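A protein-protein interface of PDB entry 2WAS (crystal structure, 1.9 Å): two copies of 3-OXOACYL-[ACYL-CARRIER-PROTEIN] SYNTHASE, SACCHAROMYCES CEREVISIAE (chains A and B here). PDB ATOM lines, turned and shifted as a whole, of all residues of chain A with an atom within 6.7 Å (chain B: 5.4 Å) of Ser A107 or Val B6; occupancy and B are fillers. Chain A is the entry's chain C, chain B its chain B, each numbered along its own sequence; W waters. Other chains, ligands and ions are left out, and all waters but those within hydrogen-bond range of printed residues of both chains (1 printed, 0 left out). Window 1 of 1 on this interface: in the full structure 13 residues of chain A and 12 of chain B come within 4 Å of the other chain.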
ATOM      1  N   VAL A   6      37.871 -16.711  23.973  1.00  0.00           N
ATOM      2  CA  VAL A   6      37.293 -15.826  24.979  1.00  0.00           C
ATOM      3  C   VAL A   6      37.738 -14.391  24.703  1.00  0.00           C
ATOM      4  O   VAL A   6      38.856 -14.140  24.252  1.00  0.00           O
ATOM      5  CB  VAL A   6      37.667 -16.257  26.462  1.00  0.00           C
ATOM      6  CG1 VAL A   6      39.155 -16.110  26.728  1.00  0.00           C
ATOM      7  CG2 VAL A   6      36.884 -15.455  27.484  1.00  0.00           C
ATOM      8  N   GLY A  46      29.134  -6.120  24.231  1.00  0.00           N
ATOM      9  CA  GLY A  46      28.884  -7.544  24.295  1.00  0.00           C
ATOM     10  C   GLY A  46      28.927  -8.259  22.949  1.00  0.00           C
ATOM     11  O   GLY A  46      29.511  -9.328  22.818  1.00  0.00           O
ATOM     12  N   SER A  49      32.521  -8.419  21.883  1.00  0.00           N
ATOM     13  CA  SER A  49      33.255  -9.501  22.545  1.00  0.00           C
ATOM     14  C   SER A  49      32.947 -10.845  21.917  1.00  0.00           C
ATOM     15  O   SER A  49      33.810 -11.703  21.815  1.00  0.00           O
ATOM     16  CB  SER A  49      32.907  -9.564  24.030  1.00  0.00           C
ATOM     17  OG  SER A  49      33.128  -8.292  24.618  1.00  0.00           O
ATOM     18  N   ARG A  76      20.939 -11.996  17.951  1.00  0.00           N
ATOM     19  CA  ARG A  76      20.412 -11.901  19.298  1.00  0.00           C
ATOM     20  C   ARG A  76      18.924 -11.569  19.289  1.00  0.00           C
ATOM     21  O   ARG A  76      18.473 -10.649  18.605  1.00  0.00           O
ATOM     22  CB  ARG A  76      21.201 -10.865  20.103  1.00  0.00           C
ATOM     23  CG  ARG A  76      22.724 -11.115  20.081  1.00  0.00           C
ATOM     24  CD  ARG A  76      23.544 -10.022  20.782  1.00  0.00           C
ATOM     25  NE  ARG A  76      23.516 -10.111  22.242  1.00  0.00           N
ATOM     26  CZ  ARG A  76      24.258  -9.365  23.058  1.00  0.00           C
ATOM     27  NH1 ARG A  76      25.106  -8.464  22.569  1.00  0.00           N
ATOM     28  NH2 ARG A  76      24.163  -9.521  24.370  1.00  0.00           N
ATOM     29  N   VAL A 104      28.170 -19.510  21.092  1.00  0.00           N
ATOM     30  CA  VAL A 104      28.696 -18.366  21.806  1.00  0.00           C
ATOM     31  C   VAL A 104      27.776 -18.014  22.975  1.00  0.00           C
ATOM     32  O   VAL A 104      26.558 -18.189  22.904  1.00  0.00           O
ATOM     33  CB  VAL A 104      28.886 -17.148  20.842  1.00  0.00           C
ATOM     34  CG1 VAL A 104      27.558 -16.493  20.492  1.00  0.00           C
ATOM     35  CG2 VAL A 104      29.842 -16.121  21.422  1.00  0.00           C
ATOM     36  N   SER A 105      28.360 -17.554  24.070  1.00  0.00           N
ATOM     37  CA  SER A 105      27.582 -17.002  25.169  1.00  0.00           C
ATOM     38  C   SER A 105      28.178 -15.653  25.552  1.00  0.00           C
ATOM     39  O   SER A 105      29.381 -15.458  25.437  1.00  0.00           O
ATOM     40  CB  SER A 105      27.578 -17.955  26.359  1.00  0.00           C
ATOM     41  OG  SER A 105      26.681 -17.520  27.354  1.00  0.00           O
ATOM     42  N   ILE A 106      27.334 -14.732  26.014  1.00  0.00           N
ATOM     43  CA  ILE A 106      27.728 -13.356  26.290  1.00  0.00           C
ATOM     44  C   ILE A 106      27.256 -12.932  27.667  1.00  0.00           C
ATOM     45  O   ILE A 106      26.164 -13.312  28.097  1.00  0.00           O
ATOM     46  CB  ILE A 106      27.113 -12.385  25.257  1.00  0.00           C
ATOM     47  CG1 ILE A 106      27.445 -12.835  23.851  1.00  0.00           C
ATOM     48  CG2 ILE A 106      27.599 -10.984  25.476  1.00  0.00           C
ATOM     49  CD1 ILE A 106      26.637 -12.142  22.819  1.00  0.00           C
ATOM     50  N   SER A 107      28.069 -12.150  28.369  1.00  0.00           N
ATOM     51  CA  SER A 107      27.666 -11.592  29.649  1.00  0.00           C
ATOM     52  C   SER A 107      28.354 -10.261  29.862  1.00  0.00           C
ATOM     53  O   SER A 107      29.431 -10.020  29.360  1.00  0.00           O
ATOM     54  CB  SER A 107      28.020 -12.550  30.799  1.00  0.00           C
ATOM     55  OG  SER A 107      27.319 -12.219  31.996  1.00  0.00           O
ATOM     56  N   HIS A 108      27.719  -9.399  30.644  1.00  0.00           N
ATOM     57  CA  HIS A 108      28.370  -8.182  31.119  1.00  0.00           C
ATOM     58  C   HIS A 108      27.905  -7.791  32.505  1.00  0.00           C
ATOM     59  O   HIS A 108      26.883  -8.276  32.994  1.00  0.00           O
ATOM     60  CB  HIS A 108      28.152  -7.031  30.130  1.00  0.00           C
ATOM     61  CG  HIS A 108      26.728  -6.579  30.028  1.00  0.00           C
ATOM     62  ND1 HIS A 108      26.184  -5.639  30.867  1.00  0.00           N
ATOM     63  CD2 HIS A 108      25.737  -6.959  29.186  1.00  0.00           C
ATOM     64  CE1 HIS A 108      24.914  -5.447  30.544  1.00  0.00           C
ATOM     65  NE2 HIS A 108      24.625  -6.225  29.523  1.00  0.00           N
ATOM     66  N   ASP A 109      28.679  -6.923  33.133  1.00  0.00           N
ATOM     67  CA  ASP A 109      28.249  -6.216  34.329  1.00  0.00           C
ATOM     68  C   ASP A 109      28.467  -4.714  34.092  1.00  0.00           C
ATOM     69  O   ASP A 109      28.426  -4.255  32.949  1.00  0.00           O
ATOM     70  CB  ASP A 109      29.014  -6.719  35.567  1.00  0.00           C
ATOM     71  CG  ASP A 109      30.536  -6.653  35.415  1.00  0.00           C
ATOM     72  OD1 ASP A 109      31.073  -5.801  34.696  1.00  0.00           O
ATOM     73  OD2 ASP A 109      31.224  -7.473  36.052  1.00  0.00           O
ATOM     74  N   GLN A 112      32.516  -4.473  32.433  1.00  0.00           N
ATOM     75  CA  GLN A 112      33.036  -5.111  31.234  1.00  0.00           C
ATOM     76  C   GLN A 112      32.123  -6.195  30.718  1.00  0.00           C
ATOM     77  O   GLN A 112      31.218  -6.659  31.418  1.00  0.00           O
ATOM     78  CB  GLN A 112      34.411  -5.679  31.531  1.00  0.00           C
ATOM     79  CG  GLN A 112      34.357  -6.913  32.405  1.00  0.00           C
ATOM     80  CD  GLN A 112      35.735  -7.284  32.933  1.00  0.00           C
ATOM     81  OE1 GLN A 112      36.470  -6.419  33.433  1.00  0.00           O
ATOM     82  NE2 GLN A 112      36.094  -8.576  32.833  1.00  0.00           N
ATOM     83  N   ALA A 113      32.349  -6.586  29.472  1.00  0.00           N
ATOM     84  CA  ALA A 113      31.576  -7.663  28.871  1.00  0.00           C
ATOM     85  C   ALA A 113      32.534  -8.782  28.607  1.00  0.00           C
ATOM     86  O   ALA A 113      33.718  -8.537  28.352  1.00  0.00           O
ATOM     87  CB  ALA A 113      30.930  -7.232  27.587  1.00  0.00           C
ATOM     88  N   VAL A 114      32.022 -10.007  28.697  1.00  0.00           N
ATOM     89  CA  VAL A 114      32.793 -11.205  28.409  1.00  0.00           C
ATOM     90  C   VAL A 114      32.016 -12.085  27.442  1.00  0.00           C
ATOM     91  O   VAL A 114      30.798 -12.170  27.514  1.00  0.00           O
ATOM     92  CB  VAL A 114      33.096 -12.002  29.680  1.00  0.00           C
ATOM     93  CG1 VAL A 114      34.021 -11.221  30.587  1.00  0.00           C
ATOM     94  CG2 VAL A 114      31.811 -12.339  30.415  1.00  0.00           C
ATOM     95  N   ALA A 115      32.715 -12.740  26.531  1.00  0.00           N
ATOM     96  CA  ALA A 115      32.068 -13.706  25.674  1.00  0.00           C
ATOM     97  C   ALA A 115      32.969 -14.933  25.553  1.00  0.00           C
ATOM     98  O   ALA A 115      34.198 -14.828  25.523  1.00  0.00           O
ATOM     99  CB  ALA A 115      31.738 -13.091  24.330  1.00  0.00           C
ATOM    100  N   VAL A 116      32.355 -16.104  25.532  1.00  0.00           N
ATOM    101  CA  VAL A 116      33.099 -17.335  25.321  1.00  0.00           C
ATOM    102  C   VAL A 116      32.470 -18.113  24.153  1.00  0.00           C
ATOM    103  O   VAL A 116      31.256 -18.258  24.067  1.00  0.00           O
ATOM    104  CB  VAL A 116      33.113 -18.188  26.605  1.00  0.00           C
ATOM    105  CG1 VAL A 116      33.845 -19.539  26.382  1.00  0.00           C
ATOM    106  CG2 VAL A 116      33.734 -17.407  27.760  1.00  0.00           C
ATOM    107  N   VAL B   4      27.174 -23.707  25.233  1.00  0.00           N
ATOM    108  CA  VAL B   4      28.120 -22.945  26.052  1.00  0.00           C
ATOM    109  C   VAL B   4      27.393 -21.833  26.788  1.00  0.00           C
ATOM    110  O   VAL B   4      26.451 -21.259  26.256  1.00  0.00           O
ATOM    111  CB  VAL B   4      29.268 -22.346  25.208  1.00  0.00           C
ATOM    112  CG1 VAL B   4      28.721 -21.339  24.234  1.00  0.00           C
ATOM    113  CG2 VAL B   4      30.317 -21.690  26.095  1.00  0.00           C
ATOM    114  N   GLY B   5      27.819 -21.539  28.012  1.00  0.00           N
ATOM    115  CA  GLY B   5      27.230 -20.451  28.761  1.00  0.00           C
ATOM    116  C   GLY B   5      28.288 -19.718  29.541  1.00  0.00           C
ATOM    117  O   GLY B   5      29.208 -20.337  30.042  1.00  0.00           O
ATOM    118  N   VAL B   6      28.171 -18.391  29.628  1.00  0.00           N
ATOM    119  CA  VAL B   6      29.101 -17.605  30.445  1.00  0.00           C
ATOM    120  C   VAL B   6      28.290 -16.661  31.318  1.00  0.00           C
ATOM    121  O   VAL B   6      27.222 -16.213  30.917  1.00  0.00           O
ATOM    122  CB  VAL B   6      30.212 -16.863  29.616  1.00  0.00           C
ATOM    123  CG1 VAL B   6      29.627 -15.798  28.708  1.00  0.00           C
ATOM    124  CG2 VAL B   6      31.242 -16.232  30.548  1.00  0.00           C
ATOM    125  N   ASP B   7      28.774 -16.412  32.531  1.00  0.00           N
ATOM    126  CA  ASP B   7      28.159 -15.431  33.418  1.00  0.00           C
ATOM    127  C   ASP B   7      29.217 -14.719  34.266  1.00  0.00           C
ATOM    128  O   ASP B   7      30.115 -15.332  34.818  1.00  0.00           O
ATOM    129  CB  ASP B   7      27.072 -16.065  34.293  1.00  0.00           C
ATOM    130  CG  ASP B   7      26.197 -15.034  34.975  1.00  0.00           C
ATOM    131  OD1 ASP B   7      25.350 -14.427  34.304  1.00  0.00           O
ATOM    132  OD2 ASP B   7      26.341 -14.830  36.186  1.00  0.00           O
ATOM    133  N   VAL B   8      29.097 -13.404  34.335  1.00  0.00           N
ATOM    134  CA  VAL B   8      30.012 -12.567  35.084  1.00  0.00           C
ATOM    135  C   VAL B   8      29.140 -11.775  36.094  1.00  0.00           C
ATOM    136  O   VAL B   8      28.048 -11.297  35.749  1.00  0.00           O
ATOM    137  CB  VAL B   8      30.817 -11.688  34.093  1.00  0.00           C
ATOM    138  CG1 VAL B   8      29.934 -10.630  33.474  1.00  0.00           C
ATOM    139  CG2 VAL B   8      31.967 -11.054  34.768  1.00  0.00           C
ATOM    140  N   ALA B  53      25.474 -19.410  34.249  1.00  0.00           N
ATOM    141  CA  ALA B  53      26.219 -19.993  33.126  1.00  0.00           C
ATOM    142  C   ALA B  53      25.672 -21.361  32.704  1.00  0.00           C
ATOM    143  O   ALA B  53      25.477 -21.619  31.524  1.00  0.00           O
ATOM    144  CB  ALA B  53      27.682 -20.126  33.483  1.00  0.00           C
ATOM    145  N   LYS B  56      22.267 -21.096  31.060  1.00  0.00           N
ATOM    146  CA  LYS B  56      22.455 -20.541  29.729  1.00  0.00           C
ATOM    147  C   LYS B  56      22.907 -21.587  28.707  1.00  0.00           C
ATOM    148  O   LYS B  56      22.456 -21.580  27.544  1.00  0.00           O
ATOM    149  CB  LYS B  56      23.473 -19.416  29.765  1.00  0.00           C
ATOM    150  CG  LYS B  56      22.996 -18.140  30.400  1.00  0.00           C
ATOM    151  CD  LYS B  56      23.712 -17.004  29.734  1.00  0.00           C
ATOM    152  CE  LYS B  56      23.857 -15.839  30.641  1.00  0.00           C
ATOM    153  NZ  LYS B  56      24.765 -14.832  30.030  1.00  0.00           N
ATOM    154  N   ALA B 115      31.890 -17.439  35.353  1.00  0.00           N
ATOM    155  CA  ALA B 115      31.701 -18.851  35.244  1.00  0.00           C
ATOM    156  C   ALA B 115      31.438 -19.197  33.791  1.00  0.00           C
ATOM    157  O   ALA B 115      30.805 -18.444  33.071  1.00  0.00           O
ATOM    158  CB  ALA B 115      30.570 -19.293  36.139  1.00  0.00           C
ATOM    159  N   VAL B 116      31.984 -20.323  33.359  1.00  0.00           N
ATOM    160  CA  VAL B 116      31.743 -20.843  32.011  1.00  0.00           C
ATOM    161  C   VAL B 116      31.241 -22.283  32.096  1.00  0.00           C
ATOM    162  O   VAL B 116      31.804 -23.085  32.827  1.00  0.00           O
ATOM    163  CB  VAL B 116      33.016 -20.754  31.109  1.00  0.00           C
ATOM    164  CG1 VAL B 116      32.756 -21.326  29.716  1.00  0.00           C
ATOM    165  CG2 VAL B 116      33.492 -19.308  31.010  1.00  0.00           C
ATOM    166  N   ALA B 117      30.175 -22.595  31.366  1.00  0.00           N
ATOM    167  CA  ALA B 117      29.628 -23.929  31.328  1.00  0.00           C
ATOM    168  C   ALA B 117      29.558 -24.397  29.889  1.00  0.00           C
ATOM    169  O   ALA B 117      29.394 -23.595  28.968  1.00  0.00           O
ATOM    170  CB  ALA B 117      28.235 -23.943  31.956  1.00  0.00           C
HETATM  171  O   HOH W   1      24.872 -20.010  24.359  1.00  0.00           O
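N of Gly B5 sits at hydrogen-bond distance from O of Ala B117, at 2.8 Å.
The backbone carbonyl oxygen (O) of Val A116 sits at hydrogen-bond distance from the backbone NH (N) of Ser A105, 3.0 Å away.
The backbone NH (N) of Ala B115 sits at hydrogen-bond distance from the backbone carbonyl oxygen (O) of Asp B7.
O of Val B6 sits at hydrogen-bond distance from NZ of Lys B56 (3.0 Å).
The backbone carbonyl oxygen of Ser A107 is in hydrogen-bond range of the backbone NH of Val A114.
OD1 of Asp A109 is in hydrogen-bond range of N of Gln A112 (3.0 Å).
Among the printed residues, pairs that only touch across the chains: Ser A105 with Gly B5, Ser A105 with Val B4, Ser A107 with Asp B7, His A108 with Val B8, Val A104 with Val B4, Ile A106 with Val B6, Ser A107 with Val B6, Val A116 with Val B116, Ser A105 with Lys B56, Val A114 with Val B8, Asp A109 with Val B8, Val A116 with Val B6, Val A114 with Val B6 and Val A116 with Val B4.
The side-chain amino group (NZ) of Lys B56 is in hydrogen-bond range of the backbone carbonyl oxygen (O) of Ile A106 (2.8 Å).
OG of Ser A105 sits at hydrogen-bond distance from N of Val B6, 2.9 Å away.
N of Val B8 is in hydrogen-bond range of OG of Ser A107, 3.2 Å away.
Val A116 touches Val B6, but with the chains exchanged Val A6 does not touch Val B116 (6.2 Å).
Val A116 touches its own counterpart, Val B116.
Positions printed for both chains: 6, 115 and 116.
Of the 17 pairs that touch across the chains among the printed residues, 1 has its exchanged pair printed and touching as well.
Gly A46 touches none of the printed residues of chain B.
Arg A76 touches none of the printed residues of chain B.
Of chain B, only Val B6, Asp B7 and Val B8 come within 4 Å of Ser A107.
Of the printed residues of chain B, Val A116 touches Val B4 (3.99 Å), Val B6 (3.9 Å) and Val B116 (3.8 Å).
Of the printed residues of chain A, Val B4 touches Val A104, Ser A105 and Val A116.
Printed residues of chain A within 4 Å of Val B6: Ser A105 (2.9 Å), Ile A106 (3.7 Å), Ser A107 (3.8 Å), Val A114 (3.9 Å) and Val A116 (3.9 Å).
Printed residues of chain A within 4 Å of Asp B7: Ser A107 (3.6 Å).
Printed residues of chain A within 4 Å of Val B8: Ser A107, His A108, Asp A109 and Val A114.
Printed residues of chain A within 4 Å of Lys B56: Ser A105 (3.8 Å) and Ile A106 (2.8 Å).
The nearest residue of chain B that does not touch Ser A107 is Lys B56 (4.05 Å).
The nearest printed residue of chain A that does not touch Val B6 is Ala A115 (4.4 Å).
The nearest printed residue of chain B that does not touch Val A116 is Gly B5 (5.6 Å).
Water W1 bridges O of Val B4 (2.8 Å) and O of Val A104 (2.9 Å).
Hydrophobic or aromatic side chains of chain B that line the printed part of chain A: Val B4, Val B6, Val B8 and Val B116.
Of the 15 printed residues of chain A, 8 touch a printed residue of chain B.
Hydrophobic or aromatic side chains of chain A that line the printed part of chain B: Val A114 and Val A116.
Among the printed residues, no Asp or Glu carboxylate lies within 4 Å of a Lys or Arg side-chain nitrogen of the other chain.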
